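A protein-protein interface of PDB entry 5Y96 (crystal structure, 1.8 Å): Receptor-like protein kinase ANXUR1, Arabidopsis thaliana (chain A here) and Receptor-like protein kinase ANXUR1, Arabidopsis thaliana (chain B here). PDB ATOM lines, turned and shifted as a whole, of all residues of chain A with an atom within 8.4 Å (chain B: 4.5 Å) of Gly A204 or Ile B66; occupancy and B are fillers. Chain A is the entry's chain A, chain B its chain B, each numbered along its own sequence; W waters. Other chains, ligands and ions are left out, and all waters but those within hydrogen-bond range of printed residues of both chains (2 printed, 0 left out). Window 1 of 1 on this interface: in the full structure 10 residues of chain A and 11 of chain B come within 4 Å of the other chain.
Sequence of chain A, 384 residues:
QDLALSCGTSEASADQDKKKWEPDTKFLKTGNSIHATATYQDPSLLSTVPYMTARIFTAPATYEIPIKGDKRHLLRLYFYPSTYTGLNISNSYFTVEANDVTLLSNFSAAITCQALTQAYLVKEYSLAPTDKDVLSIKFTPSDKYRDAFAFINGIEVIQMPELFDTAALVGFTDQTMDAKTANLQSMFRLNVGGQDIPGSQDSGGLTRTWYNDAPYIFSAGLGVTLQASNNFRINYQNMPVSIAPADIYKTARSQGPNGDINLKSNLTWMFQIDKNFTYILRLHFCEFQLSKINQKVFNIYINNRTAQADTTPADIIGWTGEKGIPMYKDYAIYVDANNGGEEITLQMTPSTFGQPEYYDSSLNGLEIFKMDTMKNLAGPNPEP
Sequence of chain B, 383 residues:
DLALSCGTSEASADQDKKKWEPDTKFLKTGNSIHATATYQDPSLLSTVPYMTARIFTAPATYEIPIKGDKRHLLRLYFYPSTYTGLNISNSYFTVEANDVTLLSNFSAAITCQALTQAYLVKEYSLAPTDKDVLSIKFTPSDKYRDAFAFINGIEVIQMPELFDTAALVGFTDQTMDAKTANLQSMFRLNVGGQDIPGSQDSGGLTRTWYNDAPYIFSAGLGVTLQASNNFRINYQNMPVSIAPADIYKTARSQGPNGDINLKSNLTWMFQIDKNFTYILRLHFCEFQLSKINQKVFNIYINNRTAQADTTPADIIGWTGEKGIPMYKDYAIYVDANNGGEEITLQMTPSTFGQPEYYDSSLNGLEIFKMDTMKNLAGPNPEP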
ATOM      1  N   ASP A   2     -16.840   1.431 -15.430  1.00  0.00           N
ATOM      2  CA  ASP A   2     -15.940   2.269 -16.212  1.00  0.00           C
ATOM      3  C   ASP A   2     -15.048   1.427 -17.118  1.00  0.00           C
ATOM      4  O   ASP A   2     -14.555   0.366 -16.723  1.00  0.00           O
ATOM      5  CB  ASP A   2     -15.079   3.132 -15.290  1.00  0.00           C
ATOM      6  CG  ASP A   2     -15.889   4.174 -14.533  1.00  0.00           C
ATOM      7  OD1 ASP A   2     -17.124   4.240 -14.722  1.00  0.00           O
ATOM      8  OD2 ASP A   2     -15.281   4.942 -13.756  1.00  0.00           O
ATOM      9  N   LEU A  74     -19.986   9.790 -18.974  1.00  0.00           N
ATOM     10  CA  LEU A  74     -19.092  10.386 -19.952  1.00  0.00           C
ATOM     11  C   LEU A  74     -18.767   9.345 -21.013  1.00  0.00           C
ATOM     12  O   LEU A  74     -18.491   8.185 -20.693  1.00  0.00           O
ATOM     13  CB  LEU A  74     -17.796  10.868 -19.295  1.00  0.00           C
ATOM     14  CG  LEU A  74     -17.743  12.233 -18.612  1.00  0.00           C
ATOM     15  CD1 LEU A  74     -16.362  12.465 -18.013  1.00  0.00           C
ATOM     16  CD2 LEU A  74     -18.111  13.347 -19.584  1.00  0.00           C
ATOM     17  N   ILE A 158     -17.489   6.331 -18.720  1.00  0.00           N
ATOM     18  CA  ILE A 158     -17.194   6.681 -17.336  1.00  0.00           C
ATOM     19  C   ILE A 158     -18.477   7.157 -16.672  1.00  0.00           C
ATOM     20  O   ILE A 158     -19.077   8.144 -17.115  1.00  0.00           O
ATOM     21  CB  ILE A 158     -16.103   7.760 -17.242  1.00  0.00           C
ATOM     22  CG1 ILE A 158     -14.907   7.396 -18.129  1.00  0.00           C
ATOM     23  CG2 ILE A 158     -15.651   7.935 -15.811  1.00  0.00           C
ATOM     24  CD1 ILE A 158     -14.000   8.562 -18.439  1.00  0.00           C
ATOM     25  N   GLN A 159     -18.895   6.457 -15.621  1.00  0.00           N
ATOM     26  CA  GLN A 159     -20.007   6.926 -14.807  1.00  0.00           C
ATOM     27  C   GLN A 159     -19.629   8.235 -14.123  1.00  0.00           C
ATOM     28  O   GLN A 159     -18.512   8.390 -13.620  1.00  0.00           O
ATOM     29  CB  GLN A 159     -20.379   5.869 -13.764  1.00  0.00           C
ATOM     30  CG  GLN A 159     -21.718   6.097 -13.091  1.00  0.00           C
ATOM     31  CD  GLN A 159     -22.012   5.065 -12.019  1.00  0.00           C
ATOM     32  OE1 GLN A 159     -22.081   3.868 -12.297  1.00  0.00           O
ATOM     33  NE2 GLN A 159     -22.185   5.525 -10.785  1.00  0.00           N
ATOM     34  N   MET A 160     -20.559   9.186 -14.113  1.00  0.00           N
ATOM     35  CA  MET A 160     -20.277  10.509 -13.573  1.00  0.00           C
ATOM     36  C   MET A 160     -21.479  11.029 -12.802  1.00  0.00           C
ATOM     37  O   MET A 160     -22.617  10.619 -13.065  1.00  0.00           O
ATOM     38  CB  MET A 160     -19.911  11.499 -14.693  1.00  0.00           C
ATOM     39  CG  MET A 160     -21.047  11.820 -15.646  1.00  0.00           C
ATOM     40  SD  MET A 160     -20.639  13.180 -16.759  1.00  0.00           S
ATOM     41  CE  MET A 160     -20.682  14.571 -15.631  1.00  0.00           C
ATOM     42  N   PRO A 161     -21.263  11.926 -11.840  1.00  0.00           N
ATOM     43  CA  PRO A 161     -22.388  12.509 -11.102  1.00  0.00           C
ATOM     44  C   PRO A 161     -23.212  13.429 -11.991  1.00  0.00           C
ATOM     45  O   PRO A 161     -22.818  13.804 -13.096  1.00  0.00           O
ATOM     46  CB  PRO A 161     -21.720  13.293  -9.964  1.00  0.00           C
ATOM     47  CG  PRO A 161     -20.303  12.804  -9.919  1.00  0.00           C
ATOM     48  CD  PRO A 161     -19.964  12.380 -11.313  1.00  0.00           C
ATOM     49  N   LEU A 163     -23.821  16.581 -12.719  1.00  0.00           N
ATOM     50  CA  LEU A 163     -23.155  17.863 -12.535  1.00  0.00           C
ATOM     51  C   LEU A 163     -23.824  19.003 -13.294  1.00  0.00           C
ATOM     52  O   LEU A 163     -23.288  20.117 -13.307  1.00  0.00           O
ATOM     53  CB  LEU A 163     -21.689  17.757 -12.961  1.00  0.00           C
ATOM     54  CG  LEU A 163     -20.847  16.715 -12.222  1.00  0.00           C
ATOM     55  CD1 LEU A 163     -19.421  16.706 -12.751  1.00  0.00           C
ATOM     56  CD2 LEU A 163     -20.868  16.985 -10.727  1.00  0.00           C
ATOM     57  N   GLY A 199      -5.606  14.538 -17.052  1.00  0.00           N
ATOM     58  CA  GLY A 199      -6.678  13.751 -16.468  1.00  0.00           C
ATOM     59  C   GLY A 199      -6.291  13.088 -15.161  1.00  0.00           C
ATOM     60  O   GLY A 199      -7.147  12.853 -14.304  1.00  0.00           O
ATOM     61  N   GLN A 201      -4.794  14.359 -12.742  1.00  0.00           N
ATOM     62  CA  GLN A 201      -4.972  15.319 -11.660  1.00  0.00           C
ATOM     63  C   GLN A 201      -6.393  15.861 -11.579  1.00  0.00           C
ATOM     64  O   GLN A 201      -6.663  16.734 -10.751  1.00  0.00           O
ATOM     65  CB  GLN A 201      -3.985  16.481 -11.822  1.00  0.00           C
ATOM     66  CG  GLN A 201      -2.523  16.072 -11.733  1.00  0.00           C
ATOM     67  CD  GLN A 201      -1.580  17.164 -12.204  1.00  0.00           C
ATOM     68  OE1 GLN A 201      -1.923  18.347 -12.190  1.00  0.00           O
ATOM     69  NE2 GLN A 201      -0.383  16.770 -12.627  1.00  0.00           N
ATOM     70  N   ASP A 202      -7.299  15.371 -12.419  1.00  0.00           N
ATOM     71  CA  ASP A 202      -8.682  15.811 -12.379  1.00  0.00           C
ATOM     72  C   ASP A 202      -9.377  15.268 -11.134  1.00  0.00           C
ATOM     73  O   ASP A 202      -8.976  14.258 -10.552  1.00  0.00           O
ATOM     74  CB  ASP A 202      -9.424  15.358 -13.638  1.00  0.00           C
ATOM     75  CG  ASP A 202     -10.814  15.952 -13.743  1.00  0.00           C
ATOM     76  OD1 ASP A 202     -11.013  17.099 -13.282  1.00  0.00           O
ATOM     77  OD2 ASP A 202     -11.711  15.264 -14.276  1.00  0.00           O
ATOM     78  N   SER A 203     -10.436  15.957 -10.731  1.00  0.00           N
ATOM     79  CA  SER A 203     -11.215  15.564  -9.571  1.00  0.00           C
ATOM     80  C   SER A 203     -12.335  14.611  -9.983  1.00  0.00           C
ATOM     81  O   SER A 203     -12.634  14.429 -11.166  1.00  0.00           O
ATOM     82  CB  SER A 203     -11.789  16.798  -8.874  1.00  0.00           C
ATOM     83  OG  SER A 203     -12.677  17.495  -9.732  1.00  0.00           O
ATOM     84  N   GLY A 204     -12.955  13.993  -8.977  1.00  0.00           N
ATOM     85  CA  GLY A 204     -14.037  13.057  -9.205  1.00  0.00           C
ATOM     86  C   GLY A 204     -13.646  11.781  -9.910  1.00  0.00           C
ATOM     87  O   GLY A 204     -14.526  10.982 -10.243  1.00  0.00           O
ATOM     88  N   GLY A 205     -12.357  11.560 -10.146  1.00  0.00           N
ATOM     89  CA  GLY A 205     -11.935  10.421 -10.937  1.00  0.00           C
ATOM     90  C   GLY A 205     -12.386  10.471 -12.377  1.00  0.00           C
ATOM     91  O   GLY A 205     -12.391   9.438 -13.054  1.00  0.00           O
ATOM     92  N   LEU A 206     -12.751  11.651 -12.878  1.00  0.00           N
ATOM     93  CA  LEU A 206     -13.330  11.780 -14.211  1.00  0.00           C
ATOM     94  C   LEU A 206     -12.288  11.930 -15.314  1.00  0.00           C
ATOM     95  O   LEU A 206     -12.654  11.908 -16.495  1.00  0.00           O
ATOM     96  CB  LEU A 206     -14.299  12.970 -14.244  1.00  0.00           C
ATOM     97  CG  LEU A 206     -15.474  12.847 -13.270  1.00  0.00           C
ATOM     98  CD1 LEU A 206     -16.322  14.116 -13.269  1.00  0.00           C
ATOM     99  CD2 LEU A 206     -16.321  11.626 -13.607  1.00  0.00           C
ATOM    100  N   THR A 207     -11.011  12.073 -14.954  1.00  0.00           N
ATOM    101  CA  THR A 207      -9.889  12.166 -15.894  1.00  0.00           C
ATOM    102  C   THR A 207     -10.161  13.135 -17.047  1.00  0.00           C
ATOM    103  O   THR A 207      -9.779  12.890 -18.192  1.00  0.00           O
ATOM    104  CB  THR A 207      -9.490  10.783 -16.428  1.00  0.00           C
ATOM    105  OG1 THR A 207     -10.594  10.170 -17.109  1.00  0.00           O
ATOM    106  CG2 THR A 207      -9.035   9.883 -15.286  1.00  0.00           C
ATOM    107  N   ARG A 208     -10.812  14.257 -16.740  1.00  0.00           N
ATOM    108  CA  ARG A 208     -10.953  15.337 -17.708  1.00  0.00           C
ATOM    109  C   ARG A 208      -9.650  16.122 -17.810  1.00  0.00           C
ATOM    110  O   ARG A 208      -8.945  16.314 -16.816  1.00  0.00           O
ATOM    111  CB  ARG A 208     -12.081  16.293 -17.310  1.00  0.00           C
ATOM    112  CG  ARG A 208     -13.481  15.694 -17.301  1.00  0.00           C
ATOM    113  CD  ARG A 208     -14.415  16.544 -16.445  1.00  0.00           C
ATOM    114  NE  ARG A 208     -13.938  16.633 -15.067  1.00  0.00           N
ATOM    115  CZ  ARG A 208     -14.575  17.273 -14.090  1.00  0.00           C
ATOM    116  NH1 ARG A 208     -15.725  17.886 -14.331  1.00  0.00           N
ATOM    117  NH2 ARG A 208     -14.059  17.295 -12.871  1.00  0.00           N
ATOM    118  N   TYR A 236     -14.422  24.137  -0.628  1.00  0.00           N
ATOM    119  CA  TYR A 236     -15.540  23.773  -1.495  1.00  0.00           C
ATOM    120  C   TYR A 236     -16.889  23.921  -0.802  1.00  0.00           C
ATOM    121  O   TYR A 236     -17.899  24.178  -1.470  1.00  0.00           O
ATOM    122  CB  TYR A 236     -15.369  22.337  -1.994  1.00  0.00           C
ATOM    123  CG  TYR A 236     -14.438  22.185  -3.177  1.00  0.00           C
ATOM    124  CD1 TYR A 236     -13.059  22.213  -3.008  1.00  0.00           C
ATOM    125  CD2 TYR A 236     -14.938  22.002  -4.462  1.00  0.00           C
ATOM    126  CE1 TYR A 236     -12.203  22.068  -4.086  1.00  0.00           C
ATOM    127  CE2 TYR A 236     -14.088  21.860  -5.545  1.00  0.00           C
ATOM    128  CZ  TYR A 236     -12.723  21.893  -5.350  1.00  0.00           C
ATOM    129  OH  TYR A 236     -11.879  21.748  -6.425  1.00  0.00           O
ATOM    130  N   PRO A 240     -19.783  20.069  -4.952  1.00  0.00           N
ATOM    131  CA  PRO A 240     -19.049  18.814  -5.168  1.00  0.00           C
ATOM    132  C   PRO A 240     -17.680  19.066  -5.781  1.00  0.00           C
ATOM    133  O   PRO A 240     -17.529  19.867  -6.706  1.00  0.00           O
ATOM    134  CB  PRO A 240     -19.955  18.031  -6.128  1.00  0.00           C
ATOM    135  CG  PRO A 240     -21.307  18.663  -5.989  1.00  0.00           C
ATOM    136  CD  PRO A 240     -21.053  20.108  -5.696  1.00  0.00           C
ATOM    137  N   VAL A 241     -16.671  18.365  -5.257  1.00  0.00           N
ATOM    138  CA  VAL A 241     -15.329  18.498  -5.809  1.00  0.00           C
ATOM    139  C   VAL A 241     -15.268  17.987  -7.240  1.00  0.00           C
ATOM    140  O   VAL A 241     -14.356  18.353  -7.989  1.00  0.00           O
ATOM    141  CB  VAL A 241     -14.297  17.771  -4.920  1.00  0.00           C
ATOM    142  CG1 VAL A 241     -14.357  18.299  -3.495  1.00  0.00           C
ATOM    143  CG2 VAL A 241     -14.529  16.272  -4.952  1.00  0.00           C
ATOM    144  N   SER A 242     -16.233  17.155  -7.647  1.00  0.00           N
ATOM    145  CA  SER A 242     -16.277  16.672  -9.021  1.00  0.00           C
ATOM    146  C   SER A 242     -16.539  17.786 -10.025  1.00  0.00           C
ATOM    147  O   SER A 242     -16.312  17.586 -11.221  1.00  0.00           O
ATOM    148  CB  SER A 242     -17.348  15.591  -9.166  1.00  0.00           C
ATOM    149  OG  SER A 242     -16.974  14.411  -8.481  1.00  0.00           O
ATOM    150  N   ILE A 243     -17.010  18.950  -9.572  1.00  0.00           N
ATOM    151  CA  ILE A 243     -17.271  20.051 -10.497  1.00  0.00           C
ATOM    152  C   ILE A 243     -15.990  20.443 -11.226  1.00  0.00           C
ATOM    153  O   ILE A 243     -15.977  20.611 -12.452  1.00  0.00           O
ATOM    154  CB  ILE A 243     -17.887  21.247  -9.750  1.00  0.00           C
ATOM    155  CG1 ILE A 243     -19.350  20.961  -9.399  1.00  0.00           C
ATOM    156  CG2 ILE A 243     -17.778  22.521 -10.579  1.00  0.00           C
ATOM    157  CD1 ILE A 243     -20.258  20.815 -10.606  1.00  0.00           C
ATOM    158  N   ALA A 244     -14.890  20.571 -10.483  1.00  0.00           N
ATOM    159  CA  ALA A 244     -13.595  20.951 -11.035  1.00  0.00           C
ATOM    160  C   ALA A 244     -12.511  20.764  -9.980  1.00  0.00           C
ATOM    161  O   ALA A 244     -12.769  20.953  -8.784  1.00  0.00           O
ATOM    162  CB  ALA A 244     -13.608  22.402 -11.527  1.00  0.00           C
ATOM    163  N   PRO A 245     -11.296  20.397 -10.380  1.00  0.00           N
ATOM    164  CA  PRO A 245     -10.226  20.197  -9.398  1.00  0.00           C
ATOM    165  C   PRO A 245      -9.770  21.513  -8.790  1.00  0.00           C
ATOM    166  O   PRO A 245     -10.016  22.598  -9.319  1.00  0.00           O
ATOM    167  CB  PRO A 245      -9.104  19.551 -10.219  1.00  0.00           C
ATOM    168  CG  PRO A 245      -9.370  19.973 -11.622  1.00  0.00           C
ATOM    169  CD  PRO A 245     -10.862  20.070 -11.750  1.00  0.00           C
ATOM    170  N   ILE B  64     -10.055  13.582   0.609  1.00  0.00           N
ATOM    171  CA  ILE B  64      -9.309  13.085  -0.542  1.00  0.00           C
ATOM    172  C   ILE B  64     -10.287  12.887  -1.693  1.00  0.00           C
ATOM    173  O   ILE B  64     -11.241  12.108  -1.561  1.00  0.00           O
ATOM    174  CB  ILE B  64      -8.568  11.781  -0.208  1.00  0.00           C
ATOM    175  CG1 ILE B  64      -7.491  12.058   0.843  1.00  0.00           C
ATOM    176  CG2 ILE B  64      -7.952  11.197  -1.459  1.00  0.00           C
ATOM    177  CD1 ILE B  64      -6.916  10.823   1.487  1.00  0.00           C
ATOM    178  N   PRO B  65     -10.103  13.569  -2.823  1.00  0.00           N
ATOM    179  CA  PRO B  65     -11.008  13.375  -3.963  1.00  0.00           C
ATOM    180  C   PRO B  65     -10.890  11.958  -4.506  1.00  0.00           C
ATOM    181  O   PRO B  65      -9.788  11.468  -4.758  1.00  0.00           O
ATOM    182  CB  PRO B  65     -10.524  14.414  -4.984  1.00  0.00           C
ATOM    183  CG  PRO B  65      -9.726  15.401  -4.191  1.00  0.00           C
ATOM    184  CD  PRO B  65      -9.093  14.605  -3.092  1.00  0.00           C
ATOM    185  N   ILE B  66     -12.036  11.299  -4.672  1.00  0.00           N
ATOM    186  CA  ILE B  66     -12.097   9.927  -5.163  1.00  0.00           C
ATOM    187  C   ILE B  66     -13.238   9.817  -6.166  1.00  0.00           C
ATOM    188  O   ILE B  66     -14.018  10.750  -6.366  1.00  0.00           O
ATOM    189  CB  ILE B  66     -12.298   8.904  -4.025  1.00  0.00           C
ATOM    190  CG1 ILE B  66     -13.522   9.281  -3.187  1.00  0.00           C
ATOM    191  CG2 ILE B  66     -11.050   8.804  -3.160  1.00  0.00           C
ATOM    192  CD1 ILE B  66     -14.027   8.167  -2.299  1.00  0.00           C
ATOM    193  N   LYS B  67     -13.325   8.651  -6.798  1.00  0.00           N
ATOM    194  CA  LYS B  67     -14.452   8.301  -7.646  1.00  0.00           C
ATOM    195  C   LYS B  67     -15.441   7.481  -6.826  1.00  0.00           C
ATOM    196  O   LYS B  67     -15.071   6.450  -6.254  1.00  0.00           O
ATOM    197  CB  LYS B  67     -13.991   7.520  -8.874  1.00  0.00           C
ATOM    198  CG  LYS B  67     -15.050   7.419  -9.941  1.00  0.00           C
ATOM    199  CD  LYS B  67     -14.470   7.567 -11.326  1.00  0.00           C
ATOM    200  CE  LYS B  67     -15.569   7.878 -12.321  1.00  0.00           C
ATOM    201  NZ  LYS B  67     -16.624   6.827 -12.328  1.00  0.00           N
ATOM    202  N   GLY B  68     -16.694   7.938  -6.783  1.00  0.00           N
ATOM    203  CA  GLY B  68     -17.654   7.394  -5.834  1.00  0.00           C
ATOM    204  C   GLY B  68     -18.032   5.943  -6.063  1.00  0.00           C
ATOM    205  O   GLY B  68     -18.401   5.243  -5.116  1.00  0.00           O
ATOM    206  N   HIS B  72     -11.715   1.118  -2.973  1.00  0.00           N
ATOM    207  CA  HIS B  72     -10.405   1.697  -2.713  1.00  0.00           C
ATOM    208  C   HIS B  72      -9.639   0.902  -1.668  1.00  0.00           C
ATOM    209  O   HIS B  72     -10.209   0.436  -0.676  1.00  0.00           O
ATOM    210  CB  HIS B  72     -10.514   3.157  -2.243  1.00  0.00           C
ATOM    211  CG  HIS B  72     -11.001   4.094  -3.301  1.00  0.00           C
ATOM    212  ND1 HIS B  72     -12.341   4.333  -3.526  1.00  0.00           N
ATOM    213  CD2 HIS B  72     -10.329   4.840  -4.209  1.00  0.00           C
ATOM    214  CE1 HIS B  72     -12.471   5.193  -4.521  1.00  0.00           C
ATOM    215  NE2 HIS B  72     -11.265   5.515  -4.954  1.00  0.00           N
ATOM    216  N   LYS B 131     -19.596   8.645  -2.961  1.00  0.00           N
ATOM    217  CA  LYS B 131     -19.222  10.017  -2.652  1.00  0.00           C
ATOM    218  C   LYS B 131     -17.896  10.321  -3.333  1.00  0.00           C
ATOM    219  O   LYS B 131     -17.024   9.452  -3.418  1.00  0.00           O
ATOM    220  CB  LYS B 131     -19.100  10.247  -1.139  1.00  0.00           C
ATOM    221  CG  LYS B 131     -20.362   9.946  -0.347  1.00  0.00           C
ATOM    222  CD  LYS B 131     -20.160  10.247   1.132  1.00  0.00           C
ATOM    223  CE  LYS B 131     -21.344   9.784   1.966  1.00  0.00           C
ATOM    224  NZ  LYS B 131     -22.583  10.542   1.644  1.00  0.00           N
ATOM    225  N   ASP B 132     -17.744  11.551  -3.819  1.00  0.00           N
ATOM    226  CA  ASP B 132     -16.525  11.931  -4.519  1.00  0.00           C
ATOM    227  C   ASP B 132     -15.439  12.439  -3.577  1.00  0.00           C
ATOM    228  O   ASP B 132     -14.414  12.943  -4.048  1.00  0.00           O
ATOM    229  CB  ASP B 132     -16.833  12.973  -5.602  1.00  0.00           C
ATOM    230  CG  ASP B 132     -17.467  14.241  -5.053  1.00  0.00           C
ATOM    231  OD1 ASP B 132     -17.696  14.336  -3.828  1.00  0.00           O
ATOM    232  OD2 ASP B 132     -17.743  15.150  -5.865  1.00  0.00           O
ATOM    233  N   VAL B 133     -15.631  12.306  -2.265  1.00  0.00           N
ATOM    234  CA  VAL B 133     -14.623  12.661  -1.275  1.00  0.00           C
ATOM    235  C   VAL B 133     -14.524  11.529  -0.264  1.00  0.00           C
ATOM    236  O   VAL B 133     -15.543  11.076   0.268  1.00  0.00           O
ATOM    237  CB  VAL B 133     -14.956  13.986  -0.560  1.00  0.00           C
ATOM    238  CG1 VAL B 133     -14.020  14.200   0.620  1.00  0.00           C
ATOM    239  CG2 VAL B 133     -14.868  15.150  -1.529  1.00  0.00           C
ATOM    240  N   LEU B 134     -13.301  11.068  -0.006  1.00  0.00           N
ATOM    241  CA  LEU B 134     -13.029  10.131   1.077  1.00  0.00           C
ATOM    242  C   LEU B 134     -12.593  10.943   2.290  1.00  0.00           C
ATOM    243  O   LEU B 134     -11.499  11.517   2.301  1.00  0.00           O
ATOM    244  CB  LEU B 134     -11.958   9.116   0.683  1.00  0.00           C
ATOM    245  CG  LEU B 134     -11.559   8.152   1.804  1.00  0.00           C
ATOM    246  CD1 LEU B 134     -12.760   7.340   2.263  1.00  0.00           C
ATOM    247  CD2 LEU B 134     -10.423   7.235   1.364  1.00  0.00           C
ATOM    248  N   VAL B 156      -4.206   5.952  -0.702  1.00  0.00           N
ATOM    249  CA  VAL B 156      -5.531   5.673  -1.248  1.00  0.00           C
ATOM    250  C   VAL B 156      -5.347   5.208  -2.687  1.00  0.00           C
ATOM    251  O   VAL B 156      -4.779   5.937  -3.509  1.00  0.00           O
ATOM    252  CB  VAL B 156      -6.458   6.899  -1.185  1.00  0.00           C
ATOM    253  CG1 VAL B 156      -7.831   6.555  -1.743  1.00  0.00           C
ATOM    254  CG2 VAL B 156      -6.578   7.398   0.248  1.00  0.00           C
HETATM  255  O   HOH W   1     -13.266  13.799  -6.409  1.00  0.00           O
HETATM  256  O   HOH W   2     -17.743  16.704  -2.761  1.00  0.00           O
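N of Gln A159 lies within hydrogen-bond range of OD1 of Asp A2 (3.0 Å). The backbone NH (N) of Ile B66 is in hydrogen-bond range of the backbone carbonyl oxygen (O) of Asp B132, at 3.0 Å. The side-chain hydroxyl (OG) of Ser A203 lies within hydrogen-bond range of the backbone carbonyl oxygen (O) of Val A241 (2.6 Å). The backbone NH of Leu A74 lies within hydrogen-bond range of the backbone carbonyl oxygen of Ile A158 (2.6 Å). The guanidinium group (NH2) of Arg A208 sits at hydrogen-bond distance from the backbone carbonyl oxygen (O) of Ser A242, at 2.8 Å.
The side-chain carboxylate of Asp A2 lies within salt-bridge range of the side-chain amino group of Lys B67, 2.7 Å away. The side-chain hydroxyl (OG) of Ser A242 sits at hydrogen-bond distance from the side-chain carboxylate (OD2) of Asp B132 (2.8 Å). The backbone NH (N) of Val A241 lies within hydrogen-bond range of the side-chain carboxylate (OD2) of Asp B132, at 3.4 Å. NZ of Lys B67 is in hydrogen-bond range of O of Gln A159 (2.8 Å).
Water W1 lies within hydrogen-bond range of the backbone NH of Gly A204, the backbone carbonyl oxygen of Asp B132 and the backbone carbonyl oxygen of Ile B66. Water W2 lies within hydrogen-bond range of the side-chain carboxylate (OD1) of Asp B132 and the backbone NH (N) of Val A241.
CG2 of Ile A158 touches CE of Lys B67, 3.5 Å away. CA of Gly A204 touches O of Ile B66, at 3.7 Å. CD of Lys B67 touches O of Gly A204, at 3.6 Å. Gly A205 touches Lys B67 (O to CD, 3.3 Å). CB of Pro A240 touches OD2 of Asp B132, 3.6 Å away. CG2 of Val A241 touches CG2 of Val B133, at 3.6 Å.
Hydrophobic or aromatic side chains of chain B that line the printed part of chain A: Val B133. Along chain B the printed residues that touch a printed residue of chain A span positions 66 to 133. Printed residues of chain A that touch a printed residue of chain B: Asp A2, Ile A158, Gln A159, Gly A204, Gly A205, Pro A240, Val A241 and Ser A242. Along chain A the printed residues that touch a printed residue of chain B span positions 2 to 242. Among the printed residues, 10 pairs touch across the chains. Among the printed residues, Asp or Glu carboxylates within 4 Å of a Lys or Arg side-chain nitrogen of the other chain: Asp A2 with Lys B67.
Leu A74 touches none of the printed residues of chain B. Gly A204 touches just these residues of chain B: Ile B66 (3.7 Å) and Lys B67 (3.6 Å). Of the printed residues of chain B, Val A241 touches Asp B132 and Val B133. Of chain A, only Gly A204 comes within 4 Å of Ile B66. Printed residues of chain A within 4 Å of Lys B67: Asp A2, Ile A158, Gln A159, Gly A204 and Gly A205. Printed residues of chain A within 4 Å of Val B133: Val A241. Leu B134 touches none of the printed residues of chain A. The nearest residue of chain A that does not touch Ile B66 is Gly A205 (4.2 Å). The nearest printed residue of chain B that does not touch Pro A240 is Val B133 (6.4 Å).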
